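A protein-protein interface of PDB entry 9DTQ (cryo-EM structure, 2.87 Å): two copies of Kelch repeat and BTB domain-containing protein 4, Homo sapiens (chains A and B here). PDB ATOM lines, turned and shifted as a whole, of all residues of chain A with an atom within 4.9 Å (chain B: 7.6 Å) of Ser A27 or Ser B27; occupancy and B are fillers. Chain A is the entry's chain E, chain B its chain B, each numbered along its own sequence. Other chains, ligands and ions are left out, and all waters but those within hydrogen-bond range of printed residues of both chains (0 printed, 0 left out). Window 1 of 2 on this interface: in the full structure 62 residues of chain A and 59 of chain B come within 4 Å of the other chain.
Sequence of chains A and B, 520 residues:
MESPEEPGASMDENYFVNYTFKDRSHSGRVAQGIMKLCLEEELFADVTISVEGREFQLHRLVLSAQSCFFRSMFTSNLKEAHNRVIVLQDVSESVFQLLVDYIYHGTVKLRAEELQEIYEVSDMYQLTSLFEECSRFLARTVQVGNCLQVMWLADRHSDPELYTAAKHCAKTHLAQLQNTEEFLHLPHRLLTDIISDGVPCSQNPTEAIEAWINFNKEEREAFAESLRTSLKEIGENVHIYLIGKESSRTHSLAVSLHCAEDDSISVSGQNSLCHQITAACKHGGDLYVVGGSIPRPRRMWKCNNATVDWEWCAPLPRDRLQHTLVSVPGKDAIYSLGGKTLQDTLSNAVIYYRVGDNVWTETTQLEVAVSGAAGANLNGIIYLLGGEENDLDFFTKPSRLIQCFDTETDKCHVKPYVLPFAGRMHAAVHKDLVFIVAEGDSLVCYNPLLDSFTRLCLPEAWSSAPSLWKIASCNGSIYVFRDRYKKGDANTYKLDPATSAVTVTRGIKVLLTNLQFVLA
NE2 of Gln B66 sits close to NE of Arg A29. The side-chain amide oxygen (OE1) of Gln B66 is in hydrogen-bond range of a ring nitrogen (ND1) of His A26 (3.4 Å).
The side-chain hydroxyl (OG) of Ser A25 lies within hydrogen-bond range of the guanidinium group (NH1) of Arg A29 (3.1 Å).
Among the printed residues, merely in contact across the chains: His A26 with Gly B106, Ser A27 with Ser B27, Ser A27 with Ala B31, Val A30 with Gln B66 and Ala A31 with Ser B27.
Printed residues of chain B within 4 Å of His A26: Gln B66 (3.4 Å) and Gly B106 (3.8 Å). Of the printed residues of chain B, Ser A27 touches Ser B27 and Ala B31. No residue of chain B comes within 4 Å of Gly A28. Of the printed residues of chain B, Val A30 touches Gln B66 (3.2 Å). Of the printed residues of chain A, Ser B27 touches Ser A27 and Ala A31. Of the printed residues of chain A, Ala B31 touches Ser A27 (3.7 Å). Of the printed residues of chain A, Gln B66 touches His A26, Arg A29 and Val A30. The nearest printed residue of chain A that does not touch Ser B27 is Gly A28 (4.5 Å). The nearest printed residue of chain B that does not touch Val A30 is Val B30 (4.3 Å).
Hydrophobic or aromatic side chains of chain B that line the printed part of chain A: Ala B31. Printed residues of chain A that touch a printed residue of chain B: His A26, Ser A27, Arg A29, Val A30 and Ala A31. Hydrophobic or aromatic side chains of chain A within 4 Å of the printed part of chain B: His A26, Val A30 and Ala A31. Among the printed residues, 7 pairs touch across the chains.
Ser B27 touches its own counterpart, Ser A27. Ser A27 touches Ala B31, and with the chains exchanged Ala A31 touches Ser B27. Positions printed for both chains: 24, 25, 26, 27, 28, 29, 30 and 31.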
ATOM      1  N   ARG A  24      10.875 -14.458  25.670  1.00  0.00           N
ATOM      2  CA  ARG A  24       9.688 -14.023  26.391  1.00  0.00           C
ATOM      3  C   ARG A  24      10.013 -13.334  27.708  1.00  0.00           C
ATOM      4  O   ARG A  24       9.113 -12.754  28.324  1.00  0.00           O
ATOM      5  CB  ARG A  24       8.763 -15.215  26.644  1.00  0.00           C
ATOM      6  CG  ARG A  24       7.711 -15.413  25.564  1.00  0.00           C
ATOM      7  CD  ARG A  24       7.441 -16.887  25.313  1.00  0.00           C
ATOM      8  NE  ARG A  24       7.285 -17.182  23.893  1.00  0.00           N
ATOM      9  CZ  ARG A  24       8.263 -17.603  23.103  1.00  0.00           C
ATOM     10  NH1 ARG A  24       9.489 -17.793  23.561  1.00  0.00           N
ATOM     11  NH2 ARG A  24       8.004 -17.842  21.820  1.00  0.00           N
ATOM     12  N   SER A  25      11.267 -13.375  28.149  1.00  0.00           N
ATOM     13  CA  SER A  25      11.700 -12.696  29.360  1.00  0.00           C
ATOM     14  C   SER A  25      12.441 -11.397  29.070  1.00  0.00           C
ATOM     15  O   SER A  25      13.066 -10.837  29.974  1.00  0.00           O
ATOM     16  CB  SER A  25      12.580 -13.625  30.196  1.00  0.00           C
ATOM     17  OG  SER A  25      13.773 -13.952  29.508  1.00  0.00           O
ATOM     18  N   HIS A  26      12.384 -10.908  27.830  1.00  0.00           N
ATOM     19  CA  HIS A  26      13.143  -9.719  27.458  1.00  0.00           C
ATOM     20  C   HIS A  26      12.594  -8.470  28.136  1.00  0.00           C
ATOM     21  O   HIS A  26      13.356  -7.670  28.691  1.00  0.00           O
ATOM     22  CB  HIS A  26      13.134  -9.557  25.937  1.00  0.00           C
ATOM     23  CG  HIS A  26      13.411  -8.160  25.474  1.00  0.00           C
ATOM     24  ND1 HIS A  26      14.681  -7.631  25.418  1.00  0.00           N
ATOM     25  CD2 HIS A  26      12.578  -7.185  25.038  1.00  0.00           C
ATOM     26  CE1 HIS A  26      14.620  -6.389  24.974  1.00  0.00           C
ATOM     27  NE2 HIS A  26      13.357  -6.094  24.735  1.00  0.00           N
ATOM     28  N   SER A  27      11.273  -8.282  28.097  1.00  0.00           N
ATOM     29  CA  SER A  27      10.677  -7.052  28.614  1.00  0.00           C
ATOM     30  C   SER A  27      10.839  -6.939  30.124  1.00  0.00           C
ATOM     31  O   SER A  27      11.166  -5.863  30.639  1.00  0.00           O
ATOM     32  CB  SER A  27       9.203  -6.986  28.224  1.00  0.00           C
ATOM     33  OG  SER A  27       8.549  -8.209  28.504  1.00  0.00           O
ATOM     34  N   GLY A  28      10.609  -8.033  30.852  1.00  0.00           N
ATOM     35  CA  GLY A  28      10.791  -7.999  32.294  1.00  0.00           C
ATOM     36  C   GLY A  28      12.230  -7.740  32.692  1.00  0.00           C
ATOM     37  O   GLY A  28      12.499  -6.984  33.628  1.00  0.00           O
ATOM     38  N   ARG A  29      13.174  -8.366  31.987  1.00  0.00           N
ATOM     39  CA  ARG A  29      14.589  -8.135  32.261  1.00  0.00           C
ATOM     40  C   ARG A  29      14.978  -6.690  31.974  1.00  0.00           C
ATOM     41  O   ARG A  29      15.726  -6.078  32.745  1.00  0.00           O
ATOM     42  CB  ARG A  29      15.439  -9.100  31.435  1.00  0.00           C
ATOM     43  CG  ARG A  29      16.928  -8.820  31.464  1.00  0.00           C
ATOM     44  CD  ARG A  29      17.707  -9.964  30.839  1.00  0.00           C
ATOM     45  NE  ARG A  29      17.405 -10.114  29.421  1.00  0.00           N
ATOM     46  CZ  ARG A  29      16.765 -11.150  28.895  1.00  0.00           C
ATOM     47  NH1 ARG A  29      16.356 -12.160  29.642  1.00  0.00           N
ATOM     48  NH2 ARG A  29      16.533 -11.171  27.587  1.00  0.00           N
ATOM     49  N   VAL A  30      14.471  -6.127  30.874  1.00  0.00           N
ATOM     50  CA  VAL A  30      14.751  -4.732  30.545  1.00  0.00           C
ATOM     51  C   VAL A  30      14.201  -3.809  31.626  1.00  0.00           C
ATOM     52  O   VAL A  30      14.876  -2.875  32.072  1.00  0.00           O
ATOM     53  CB  VAL A  30      14.176  -4.382  29.159  1.00  0.00           C
ATOM     54  CG1 VAL A  30      13.800  -2.910  29.083  1.00  0.00           C
ATOM     55  CG2 VAL A  30      15.173  -4.724  28.074  1.00  0.00           C
ATOM     56  N   ALA A  31      12.966  -4.062  32.068  1.00  0.00           N
ATOM     57  CA  ALA A  31      12.358  -3.217  33.091  1.00  0.00           C
ATOM     58  C   ALA A  31      13.122  -3.302  34.407  1.00  0.00           C
ATOM     59  O   ALA A  31      13.394  -2.279  35.048  1.00  0.00           O
ATOM     60  CB  ALA A  31      10.896  -3.611  33.290  1.00  0.00           C
ATOM     61  N   ASP B  23       0.977  -1.025  38.116  1.00  0.00           N
ATOM     62  CA  ASP B  23       0.612  -1.164  36.713  1.00  0.00           C
ATOM     63  C   ASP B  23       1.225  -2.444  36.159  1.00  0.00           C
ATOM     64  O   ASP B  23       2.452  -2.582  36.118  1.00  0.00           O
ATOM     65  CB  ASP B  23       1.082   0.051  35.917  1.00  0.00           C
ATOM     66  CG  ASP B  23       0.205   0.334  34.718  1.00  0.00           C
ATOM     67  OD1 ASP B  23      -0.758  -0.423  34.492  1.00  0.00           O
ATOM     68  OD2 ASP B  23       0.478   1.319  34.002  1.00  0.00           O
ATOM     69  N   ARG B  24       0.372  -3.376  35.736  1.00  0.00           N
ATOM     70  CA  ARG B  24       0.835  -4.644  35.190  1.00  0.00           C
ATOM     71  C   ARG B  24       1.327  -4.531  33.755  1.00  0.00           C
ATOM     72  O   ARG B  24       1.995  -5.452  33.273  1.00  0.00           O
ATOM     73  CB  ARG B  24      -0.283  -5.686  35.263  1.00  0.00           C
ATOM     74  CG  ARG B  24      -0.509  -6.248  36.654  1.00  0.00           C
ATOM     75  CD  ARG B  24      -1.227  -7.592  36.605  1.00  0.00           C
ATOM     76  NE  ARG B  24      -2.668  -7.470  36.400  1.00  0.00           N
ATOM     77  CZ  ARG B  24      -3.505  -6.825  37.203  1.00  0.00           C
ATOM     78  NH1 ARG B  24      -3.095  -6.261  38.328  1.00  0.00           N
ATOM     79  NH2 ARG B  24      -4.793  -6.757  36.875  1.00  0.00           N
ATOM     80  N   SER B  25       1.020  -3.433  33.065  1.00  0.00           N
ATOM     81  CA  SER B  25       1.449  -3.220  31.691  1.00  0.00           C
ATOM     82  C   SER B  25       2.678  -2.326  31.597  1.00  0.00           C
ATOM     83  O   SER B  25       2.998  -1.835  30.511  1.00  0.00           O
ATOM     84  CB  SER B  25       0.302  -2.631  30.870  1.00  0.00           C
ATOM     85  OG  SER B  25      -0.173  -1.432  31.454  1.00  0.00           O
ATOM     86  N   HIS B  26       3.369  -2.103  32.717  1.00  0.00           N
ATOM     87  CA  HIS B  26       4.504  -1.187  32.725  1.00  0.00           C
ATOM     88  C   HIS B  26       5.677  -1.741  31.925  1.00  0.00           C
ATOM     89  O   HIS B  26       6.259  -1.036  31.094  1.00  0.00           O
ATOM     90  CB  HIS B  26       4.924  -0.896  34.166  1.00  0.00           C
ATOM     91  CG  HIS B  26       6.322  -0.374  34.296  1.00  0.00           C
ATOM     92  ND1 HIS B  26       6.655   0.938  34.039  1.00  0.00           N
ATOM     93  CD2 HIS B  26       7.472  -0.989  34.660  1.00  0.00           C
ATOM     94  CE1 HIS B  26       7.950   1.108  34.235  1.00  0.00           C
ATOM     95  NE2 HIS B  26       8.469  -0.045  34.613  1.00  0.00           N
ATOM     96  N   SER B  27       6.041  -3.005  32.167  1.00  0.00           N
ATOM     97  CA  SER B  27       7.233  -3.571  31.539  1.00  0.00           C
ATOM     98  C   SER B  27       7.079  -3.669  30.027  1.00  0.00           C
ATOM     99  O   SER B  27       8.002  -3.323  29.280  1.00  0.00           O
ATOM    100  CB  SER B  27       7.534  -4.944  32.134  1.00  0.00           C
ATOM    101  OG  SER B  27       7.734  -4.862  33.533  1.00  0.00           O
ATOM    102  N   GLY B  28       5.927  -4.146  29.558  1.00  0.00           N
ATOM    103  CA  GLY B  28       5.706  -4.234  28.125  1.00  0.00           C
ATOM    104  C   GLY B  28       5.702  -2.875  27.455  1.00  0.00           C
ATOM    105  O   GLY B  28       6.255  -2.708  26.367  1.00  0.00           O
ATOM    106  N   ARG B  29       5.075  -1.887  28.096  1.00  0.00           N
ATOM    107  CA  ARG B  29       5.066  -0.533  27.553  1.00  0.00           C
ATOM    108  C   ARG B  29       6.474   0.040  27.480  1.00  0.00           C
ATOM    109  O   ARG B  29       6.844   0.671  26.484  1.00  0.00           O
ATOM    110  CB  ARG B  29       4.165   0.361  28.403  1.00  0.00           C
ATOM    111  CG  ARG B  29       4.442   1.848  28.275  1.00  0.00           C
ATOM    112  CD  ARG B  29       3.272   2.681  28.780  1.00  0.00           C
ATOM    113  NE  ARG B  29       3.071   2.542  30.219  1.00  0.00           N
ATOM    114  CZ  ARG B  29       2.190   1.727  30.779  1.00  0.00           C
ATOM    115  NH1 ARG B  29       1.389   0.968  30.051  1.00  0.00           N
ATOM    116  NH2 ARG B  29       2.106   1.674  32.105  1.00  0.00           N
ATOM    117  N   VAL B  30       7.277  -0.179  28.523  1.00  0.00           N
ATOM    118  CA  VAL B  30       8.653   0.315  28.531  1.00  0.00           C
ATOM    119  C   VAL B  30       9.459  -0.334  27.413  1.00  0.00           C
ATOM    120  O   VAL B  30      10.180   0.341  26.670  1.00  0.00           O
ATOM    121  CB  VAL B  30       9.298   0.071  29.908  1.00  0.00           C
ATOM    122  CG1 VAL B  30      10.811   0.038  29.798  1.00  0.00           C
ATOM    123  CG2 VAL B  30       8.861   1.135  30.886  1.00  0.00           C
ATOM    124  N   ALA B  31       9.342  -1.657  27.274  1.00  0.00           N
ATOM    125  CA  ALA B  31      10.094  -2.358  26.238  1.00  0.00           C
ATOM    126  C   ALA B  31       9.677  -1.896  24.847  1.00  0.00           C
ATOM    127  O   ALA B  31      10.527  -1.635  23.988  1.00  0.00           O
ATOM    128  CB  ALA B  31       9.908  -3.867  26.388  1.00  0.00           C
ATOM    129  N   GLN B  32       8.367  -1.782  24.610  1.00  0.00           N
ATOM    130  CA  GLN B  32       7.882  -1.349  23.305  1.00  0.00           C
ATOM    131  C   GLN B  32       8.323   0.074  22.994  1.00  0.00           C
ATOM    132  O   GLN B  32       8.696   0.378  21.855  1.00  0.00           O
ATOM    133  CB  GLN B  32       6.360  -1.463  23.249  1.00  0.00           C
ATOM    134  CG  GLN B  32       5.863  -2.753  22.621  1.00  0.00           C
ATOM    135  CD  GLN B  32       4.701  -3.361  23.379  1.00  0.00           C
ATOM    136  OE1 GLN B  32       3.790  -2.654  23.813  1.00  0.00           O
ATOM    137  NE2 GLN B  32       4.727  -4.677  23.546  1.00  0.00           N
ATOM    138  N   GLY B  33       8.282   0.961  23.988  1.00  0.00           N
ATOM    139  CA  GLY B  33       8.761   2.315  23.776  1.00  0.00           C
ATOM    140  C   GLY B  33      10.240   2.362  23.456  1.00  0.00           C
ATOM    141  O   GLY B  33      10.671   3.125  22.590  1.00  0.00           O
ATOM    142  N   MET B  35      12.009  -0.031  22.001  1.00  0.00           N
ATOM    143  CA  MET B  35      12.192  -0.524  20.636  1.00  0.00           C
ATOM    144  C   MET B  35      11.778   0.526  19.612  1.00  0.00           C
ATOM    145  O   MET B  35      12.502   0.787  18.644  1.00  0.00           O
ATOM    146  CB  MET B  35      11.408  -1.820  20.418  1.00  0.00           C
ATOM    147  CG  MET B  35      11.615  -2.876  21.488  1.00  0.00           C
ATOM    148  SD  MET B  35      10.503  -4.291  21.354  1.00  0.00           S
ATOM    149  CE  MET B  35       9.759  -3.999  19.752  1.00  0.00           C
ATOM    150  N   GLN B  66      21.109  -5.187  29.732  1.00  0.00           N
ATOM    151  CA  GLN B  66      20.992  -6.496  29.102  1.00  0.00           C
ATOM    152  C   GLN B  66      22.173  -7.418  29.367  1.00  0.00           C
ATOM    153  O   GLN B  66      22.019  -8.639  29.265  1.00  0.00           O
ATOM    154  CB  GLN B  66      20.814  -6.338  27.589  1.00  0.00           C
ATOM    155  CG  GLN B  66      19.402  -5.973  27.185  1.00  0.00           C
ATOM    156  CD  GLN B  66      18.473  -7.164  27.216  1.00  0.00           C
ATOM    157  OE1 GLN B  66      17.279  -7.027  27.463  1.00  0.00           O
ATOM    158  NE2 GLN B  66      19.018  -8.343  26.958  1.00  0.00           N
ATOM    159  N   HIS B 105      15.322  -5.573  20.460  1.00  0.00           N
ATOM    160  CA  HIS B 105      13.988  -6.053  20.137  1.00  0.00           C
ATOM    161  C   HIS B 105      13.604  -7.345  20.838  1.00  0.00           C
ATOM    162  O   HIS B 105      12.409  -7.622  20.965  1.00  0.00           O
ATOM    163  CB  HIS B 105      13.852  -6.257  18.622  1.00  0.00           C
ATOM    164  CG  HIS B 105      14.223  -5.052  17.817  1.00  0.00           C
ATOM    165  ND1 HIS B 105      15.254  -5.056  16.904  1.00  0.00           N
ATOM    166  CD2 HIS B 105      13.704  -3.802  17.793  1.00  0.00           C
ATOM    167  CE1 HIS B 105      15.354  -3.860  16.350  1.00  0.00           C
ATOM    168  NE2 HIS B 105      14.425  -3.081  16.872  1.00  0.00           N
ATOM    169  N   GLY B 106      14.570  -8.135  21.293  1.00  0.00           N
ATOM    170  CA  GLY B 106      14.276  -9.385  21.959  1.00  0.00           C
ATOM    171  C   GLY B 106      14.010 -10.551  21.038  1.00  0.00           C
ATOM    172  O   GLY B 106      13.799 -11.667  21.527  1.00  0.00           O
